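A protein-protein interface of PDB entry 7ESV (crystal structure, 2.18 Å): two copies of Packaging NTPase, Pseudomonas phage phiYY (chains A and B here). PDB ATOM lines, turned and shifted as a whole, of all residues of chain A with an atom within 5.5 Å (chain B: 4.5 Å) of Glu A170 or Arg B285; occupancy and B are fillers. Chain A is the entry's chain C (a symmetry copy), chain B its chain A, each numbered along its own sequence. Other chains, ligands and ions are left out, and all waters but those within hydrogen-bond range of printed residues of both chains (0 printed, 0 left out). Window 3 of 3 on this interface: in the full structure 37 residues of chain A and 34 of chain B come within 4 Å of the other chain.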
ATOM      1  N   SER A 151     -14.028 -32.739 -12.251  1.00  0.00           N
ATOM      2  CA  SER A 151     -12.735 -32.112 -11.960  1.00  0.00           C
ATOM      3  C   SER A 151     -11.614 -33.155 -11.983  1.00  0.00           C
ATOM      4  O   SER A 151     -10.589 -32.981 -12.662  1.00  0.00           O
ATOM      5  CB  SER A 151     -12.774 -31.373 -10.611  1.00  0.00           C
ATOM      6  OG  SER A 151     -13.735 -30.326 -10.624  1.00  0.00           O
ATOM      7  N   ARG A 164     -12.768 -21.241 -16.666  1.00  0.00           N
ATOM      8  CA  ARG A 164     -13.883 -21.333 -15.736  1.00  0.00           C
ATOM      9  C   ARG A 164     -14.950 -20.312 -16.100  1.00  0.00           C
ATOM     10  O   ARG A 164     -14.662 -19.116 -16.218  1.00  0.00           O
ATOM     11  CB  ARG A 164     -13.412 -21.125 -14.298  1.00  0.00           C
ATOM     12  CG  ARG A 164     -12.533 -22.247 -13.794  1.00  0.00           C
ATOM     13  CD  ARG A 164     -13.353 -23.383 -13.223  1.00  0.00           C
ATOM     14  NE  ARG A 164     -14.002 -23.002 -11.973  1.00  0.00           N
ATOM     15  CZ  ARG A 164     -15.115 -23.563 -11.512  1.00  0.00           C
ATOM     16  NH1 ARG A 164     -15.703 -24.532 -12.201  1.00  0.00           N
ATOM     17  NH2 ARG A 164     -15.640 -23.154 -10.366  1.00  0.00           N
ATOM     18  N   PRO A 168     -19.884 -21.574  -9.693  1.00  0.00           N
ATOM     19  CA  PRO A 168     -19.536 -20.853  -8.465  1.00  0.00           C
ATOM     20  C   PRO A 168     -18.052 -20.978  -8.162  1.00  0.00           C
ATOM     21  O   PRO A 168     -17.433 -22.016  -8.409  1.00  0.00           O
ATOM     22  CB  PRO A 168     -20.391 -21.537  -7.393  1.00  0.00           C
ATOM     23  CG  PRO A 168     -20.649 -22.900  -7.937  1.00  0.00           C
ATOM     24  CD  PRO A 168     -20.770 -22.721  -9.425  1.00  0.00           C
ATOM     25  N   ALA A 169     -17.479 -19.899  -7.635  1.00  0.00           N
ATOM     26  CA  ALA A 169     -16.065 -19.897  -7.292  1.00  0.00           C
ATOM     27  C   ALA A 169     -15.780 -20.937  -6.215  1.00  0.00           C
ATOM     28  O   ALA A 169     -16.583 -21.148  -5.304  1.00  0.00           O
ATOM     29  CB  ALA A 169     -15.635 -18.509  -6.818  1.00  0.00           C
ATOM     30  N   GLU A 170     -14.663 -21.606  -6.347  1.00  0.00           N
ATOM     31  CA  GLU A 170     -14.210 -22.588  -5.398  1.00  0.00           C
ATOM     32  C   GLU A 170     -12.716 -22.580  -5.287  1.00  0.00           C
ATOM     33  O   GLU A 170     -12.041 -21.859  -5.977  1.00  0.00           O
ATOM     34  CB  GLU A 170     -14.698 -23.980  -5.743  1.00  0.00           C
ATOM     35  CG  GLU A 170     -14.426 -24.470  -7.140  1.00  0.00           C
ATOM     36  CD  GLU A 170     -15.195 -25.736  -7.453  1.00  0.00           C
ATOM     37  OE1 GLU A 170     -16.287 -25.650  -8.020  1.00  0.00           O
ATOM     38  OE2 GLU A 170     -14.735 -26.825  -7.116  1.00  0.00           O
ATOM     39  N   ARG A 171     -12.199 -23.443  -4.437  1.00  0.00           N
ATOM     40  CA  ARG A 171     -10.778 -23.598  -4.183  1.00  0.00           C
ATOM     41  C   ARG A 171      -9.927 -23.658  -5.417  1.00  0.00           C
ATOM     42  O   ARG A 171      -8.911 -23.041  -5.468  1.00  0.00           O
ATOM     43  CB  ARG A 171     -10.519 -24.854  -3.368  1.00  0.00           C
ATOM     44  CG  ARG A 171      -9.249 -24.826  -2.553  1.00  0.00           C
ATOM     45  CD  ARG A 171      -8.944 -26.134  -1.841  1.00  0.00           C
ATOM     46  NE  ARG A 171     -10.068 -26.612  -1.057  1.00  0.00           N
ATOM     47  CZ  ARG A 171     -10.033 -26.886   0.242  1.00  0.00           C
ATOM     48  NH1 ARG A 171     -11.109 -27.312   0.862  1.00  0.00           N
ATOM     49  NH2 ARG A 171      -8.927 -26.738   0.924  1.00  0.00           N
ATOM     50  N   PHE A 172     -10.335 -24.439  -6.396  1.00  0.00           N
ATOM     51  CA  PHE A 172      -9.625 -24.547  -7.639  1.00  0.00           C
ATOM     52  C   PHE A 172      -9.384 -23.217  -8.303  1.00  0.00           C
ATOM     53  O   PHE A 172      -8.342 -23.029  -8.863  1.00  0.00           O
ATOM     54  CB  PHE A 172     -10.402 -25.428  -8.587  1.00  0.00           C
ATOM     55  CG  PHE A 172      -9.640 -25.830  -9.794  1.00  0.00           C
ATOM     56  CD1 PHE A 172      -8.566 -26.678  -9.689  1.00  0.00           C
ATOM     57  CD2 PHE A 172     -10.004 -25.387 -11.029  1.00  0.00           C
ATOM     58  CE1 PHE A 172      -7.857 -27.063 -10.798  1.00  0.00           C
ATOM     59  CE2 PHE A 172      -9.306 -25.769 -12.138  1.00  0.00           C
ATOM     60  CZ  PHE A 172      -8.234 -26.607 -12.026  1.00  0.00           C
ATOM     61  N   ASP A 173     -10.332 -22.295  -8.232  1.00  0.00           N
ATOM     62  CA  ASP A 173     -10.143 -21.015  -8.909  1.00  0.00           C
ATOM     63  C   ASP A 173      -8.985 -20.219  -8.311  1.00  0.00           C
ATOM     64  O   ASP A 173      -8.407 -19.360  -8.988  1.00  0.00           O
ATOM     65  CB  ASP A 173     -11.446 -20.214  -8.861  1.00  0.00           C
ATOM     66  CG  ASP A 173     -12.614 -20.947  -9.527  1.00  0.00           C
ATOM     67  OD1 ASP A 173     -12.529 -21.238 -10.741  1.00  0.00           O
ATOM     68  OD2 ASP A 173     -13.618 -21.233  -8.843  1.00  0.00           O
ATOM     69  N   VAL A 174      -8.646 -20.520  -7.083  1.00  0.00           N
ATOM     70  CA  VAL A 174      -7.589 -19.843  -6.414  1.00  0.00           C
ATOM     71  C   VAL A 174      -6.347 -20.665  -6.513  1.00  0.00           C
ATOM     72  O   VAL A 174      -5.274 -20.172  -6.725  1.00  0.00           O
ATOM     73  CB  VAL A 174      -7.925 -19.736  -4.940  1.00  0.00           C
ATOM     74  CG1 VAL A 174      -6.723 -19.313  -4.156  1.00  0.00           C
ATOM     75  CG2 VAL A 174      -9.056 -18.786  -4.717  1.00  0.00           C
ATOM     76  N   ASP B 134     -12.923 -20.593   6.788  1.00  0.00           N
ATOM     77  CA  ASP B 134     -12.425 -20.680   5.415  1.00  0.00           C
ATOM     78  C   ASP B 134     -13.551 -20.759   4.389  1.00  0.00           C
ATOM     79  O   ASP B 134     -13.326 -21.185   3.251  1.00  0.00           O
ATOM     80  CB  ASP B 134     -11.463 -21.860   5.250  1.00  0.00           C
ATOM     81  CG  ASP B 134     -10.281 -21.779   6.197  1.00  0.00           C
ATOM     82  OD1 ASP B 134     -10.237 -20.831   7.010  1.00  0.00           O
ATOM     83  OD2 ASP B 134      -9.399 -22.659   6.131  1.00  0.00           O
ATOM     84  N   HIS B 135     -14.756 -20.357   4.789  1.00  0.00           N
ATOM     85  CA  HIS B 135     -15.881 -20.222   3.873  1.00  0.00           C
ATOM     86  C   HIS B 135     -15.475 -19.434   2.636  1.00  0.00           C
ATOM     87  O   HIS B 135     -14.896 -18.348   2.738  1.00  0.00           O
ATOM     88  CB  HIS B 135     -17.035 -19.520   4.595  1.00  0.00           C
ATOM     89  CG  HIS B 135     -18.362 -19.661   3.919  1.00  0.00           C
ATOM     90  ND1 HIS B 135     -18.586 -19.256   2.621  1.00  0.00           N
ATOM     91  CD2 HIS B 135     -19.546 -20.138   4.373  1.00  0.00           C
ATOM     92  CE1 HIS B 135     -19.846 -19.489   2.300  1.00  0.00           C
ATOM     93  NE2 HIS B 135     -20.450 -20.025   3.345  1.00  0.00           N
ATOM     94  N   MET B 136     -15.763 -19.996   1.463  1.00  0.00           N
ATOM     95  CA  MET B 136     -15.477 -19.299   0.222  1.00  0.00           C
ATOM     96  C   MET B 136     -16.299 -18.015   0.148  1.00  0.00           C
ATOM     97  O   MET B 136     -17.427 -17.960   0.651  1.00  0.00           O
ATOM     98  CB  MET B 136     -15.794 -20.186  -0.982  1.00  0.00           C
ATOM     99  CG  MET B 136     -14.676 -21.134  -1.389  1.00  0.00           C
ATOM    100  SD  MET B 136     -13.242 -20.287  -2.077  1.00  0.00           S
ATOM    101  CE  MET B 136     -13.960 -19.543  -3.536  1.00  0.00           C
ATOM    102  N   ALA B 265     -27.405 -25.557  -4.002  1.00  0.00           N
ATOM    103  CA  ALA B 265     -26.084 -25.682  -3.401  1.00  0.00           C
ATOM    104  C   ALA B 265     -24.999 -25.699  -4.468  1.00  0.00           C
ATOM    105  O   ALA B 265     -23.917 -25.136  -4.273  1.00  0.00           O
ATOM    106  CB  ALA B 265     -26.016 -26.939  -2.536  1.00  0.00           C
ATOM    107  N   ALA B 266     -25.277 -26.327  -5.613  1.00  0.00           N
ATOM    108  CA  ALA B 266     -24.310 -26.357  -6.702  1.00  0.00           C
ATOM    109  C   ALA B 266     -24.110 -24.994  -7.350  1.00  0.00           C
ATOM    110  O   ALA B 266     -23.207 -24.852  -8.182  1.00  0.00           O
ATOM    111  CB  ALA B 266     -24.739 -27.371  -7.762  1.00  0.00           C
ATOM    112  N   SER B 267     -24.919 -23.998  -6.994  1.00  0.00           N
ATOM    113  CA  SER B 267     -24.836 -22.677  -7.597  1.00  0.00           C
ATOM    114  C   SER B 267     -24.092 -21.660  -6.742  1.00  0.00           C
ATOM    115  O   SER B 267     -23.730 -20.598  -7.256  1.00  0.00           O
ATOM    116  CB  SER B 267     -26.245 -22.141  -7.890  1.00  0.00           C
ATOM    117  OG  SER B 267     -27.028 -23.100  -8.579  1.00  0.00           O
ATOM    118  N   VAL B 268     -23.851 -21.946  -5.461  1.00  0.00           N
ATOM    119  CA  VAL B 268     -23.370 -20.938  -4.523  1.00  0.00           C
ATOM    120  C   VAL B 268     -22.221 -21.494  -3.691  1.00  0.00           C
ATOM    121  O   VAL B 268     -21.874 -22.674  -3.764  1.00  0.00           O
ATOM    122  CB  VAL B 268     -24.491 -20.430  -3.593  1.00  0.00           C
ATOM    123  CG1 VAL B 268     -25.592 -19.759  -4.399  1.00  0.00           C
ATOM    124  CG2 VAL B 268     -25.048 -21.578  -2.764  1.00  0.00           C
ATOM    125  N   ALA B 269     -21.638 -20.605  -2.883  1.00  0.00           N
ATOM    126  CA  ALA B 269     -20.526 -20.982  -2.017  1.00  0.00           C
ATOM    127  C   ALA B 269     -20.982 -21.898  -0.889  1.00  0.00           C
ATOM    128  O   ALA B 269     -20.290 -22.866  -0.552  1.00  0.00           O
ATOM    129  CB  ALA B 269     -19.860 -19.729  -1.448  1.00  0.00           C
ATOM    130  N   THR B 283     -23.854 -27.362   3.457  1.00  0.00           N
ATOM    131  CA  THR B 283     -22.768 -27.622   2.523  1.00  0.00           C
ATOM    132  C   THR B 283     -22.030 -26.316   2.270  1.00  0.00           C
ATOM    133  O   THR B 283     -22.661 -25.297   1.971  1.00  0.00           O
ATOM    134  CB  THR B 283     -23.296 -28.187   1.201  1.00  0.00           C
ATOM    135  OG1 THR B 283     -24.154 -27.220   0.582  1.00  0.00           O
ATOM    136  CG2 THR B 283     -24.091 -29.460   1.445  1.00  0.00           C
ATOM    137  N   VAL B 284     -20.704 -26.340   2.390  1.00  0.00           N
ATOM    138  CA  VAL B 284     -19.893 -25.136   2.233  1.00  0.00           C
ATOM    139  C   VAL B 284     -18.641 -25.475   1.435  1.00  0.00           C
ATOM    140  O   VAL B 284     -17.924 -26.425   1.765  1.00  0.00           O
ATOM    141  CB  VAL B 284     -19.505 -24.520   3.592  1.00  0.00           C
ATOM    142  CG1 VAL B 284     -18.466 -23.426   3.406  1.00  0.00           C
ATOM    143  CG2 VAL B 284     -20.732 -23.968   4.303  1.00  0.00           C
ATOM    144  N   ARG B 285     -18.386 -24.702   0.382  1.00  0.00           N
ATOM    145  CA  ARG B 285     -17.088 -24.713  -0.276  1.00  0.00           C
ATOM    146  C   ARG B 285     -16.106 -23.880   0.533  1.00  0.00           C
ATOM    147  O   ARG B 285     -16.427 -22.773   0.976  1.00  0.00           O
ATOM    148  CB  ARG B 285     -17.193 -24.154  -1.693  1.00  0.00           C
ATOM    149  CG  ARG B 285     -18.166 -24.893  -2.576  1.00  0.00           C
ATOM    150  CD  ARG B 285     -18.361 -24.161  -3.885  1.00  0.00           C
ATOM    151  NE  ARG B 285     -19.722 -24.322  -4.379  1.00  0.00           N
ATOM    152  CZ  ARG B 285     -20.117 -25.337  -5.137  1.00  0.00           C
ATOM    153  NH1 ARG B 285     -21.376 -25.412  -5.542  1.00  0.00           N
ATOM    154  NH2 ARG B 285     -19.251 -26.277  -5.490  1.00  0.00           N
ATOM    155  N   THR B 286     -14.905 -24.415   0.729  1.00  0.00           N
ATOM    156  CA  THR B 286     -13.926 -23.792   1.605  1.00  0.00           C
ATOM    157  C   THR B 286     -12.583 -23.675   0.899  1.00  0.00           C
ATOM    158  O   THR B 286     -12.339 -24.282  -0.146  1.00  0.00           O
ATOM    159  CB  THR B 286     -13.750 -24.584   2.909  1.00  0.00           C
ATOM    160  OG1 THR B 286     -13.099 -25.831   2.628  1.00  0.00           O
ATOM    161  CG2 THR B 286     -15.094 -24.857   3.565  1.00  0.00           C
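The guanidinium group (NH2) of Arg B285 is in salt-bridge range of the side-chain carboxylate (OE1) of Glu A170, at 3.9 Å. The guanidinium group (NH1) of Arg A171 is in hydrogen-bond range of the side-chain hydroxyl (OG1) of Thr B286 (3.0 Å).
The backbone carbonyl oxygen (O) of Ala B265 is in hydrogen-bond range of the guanidinium group (NH1) of Arg B285, at 2.9 Å. The backbone carbonyl oxygen of Val B268 is in hydrogen-bond range of the guanidinium group of Arg B285 (2.8 Å). N of Arg B285 lies within hydrogen-bond range of O of Ala B269, at 2.8 Å. The backbone carbonyl oxygen of Pro A168 is in hydrogen-bond range of the guanidinium group of Arg A164 (2.9 Å). The side-chain carboxylate (OE1) of Glu A170 is in salt-bridge range of the guanidinium group (NH2) of Arg A164 (3.5 Å). The backbone NH of Glu A170 sits at hydrogen-bond distance from the side-chain carboxylate of Asp A173 (2.7 Å).
Among the printed residues, pairs that only touch across the chains: Pro A168 with Ala B266 (3.2 Å), Pro A168 with Ser B267 (3.5 Å), Ala A169 with Met B136 (3.5 Å), Pro A168 with Arg B285 (3.5 Å), Glu A170 with Met B136 (3.6 Å), Ala A169 with Arg B285 (3.8 Å) and Pro A168 with Val B268 (3.98 Å).
Of the printed residues of chain B, Pro A168 touches Ala B266, Ser B267, Val B268 and Arg B285. Of the printed residues of chain B, Ala A169 touches Met B136 and Arg B285. Glu A170 touches two residues of chain B. Of the printed residues of chain A, Ala B266 touches Pro A168. Ala B269 touches none of the printed residues of chain A. Of the printed residues of chain A, Arg B285 touches Pro A168, Ala A169 and Glu A170. The nearest printed residue of chain B that does not touch Arg A171 is Met B136 (4.1 Å).
Hydrophobic or aromatic side chains of chain A within 4 Å of the printed part of chain B: Pro A168 and Ala A169. Of the 12 printed residues of chain B, 6 touch a printed residue of chain A. Hydrophobic or aromatic side chains of chain B within 4 Å of the printed part of chain A: Met B136. Among the printed residues, 9 pairs touch across the chains. Among the printed residues, Asp or Glu carboxylates within 4 Å of a Lys or Arg side-chain nitrogen of the other chain: Glu A170 with Arg B285.
No position is printed for both chains. Of the 9 pairs that touch across the chains among the printed residues, none has its exchanged pair printed and touching as well.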
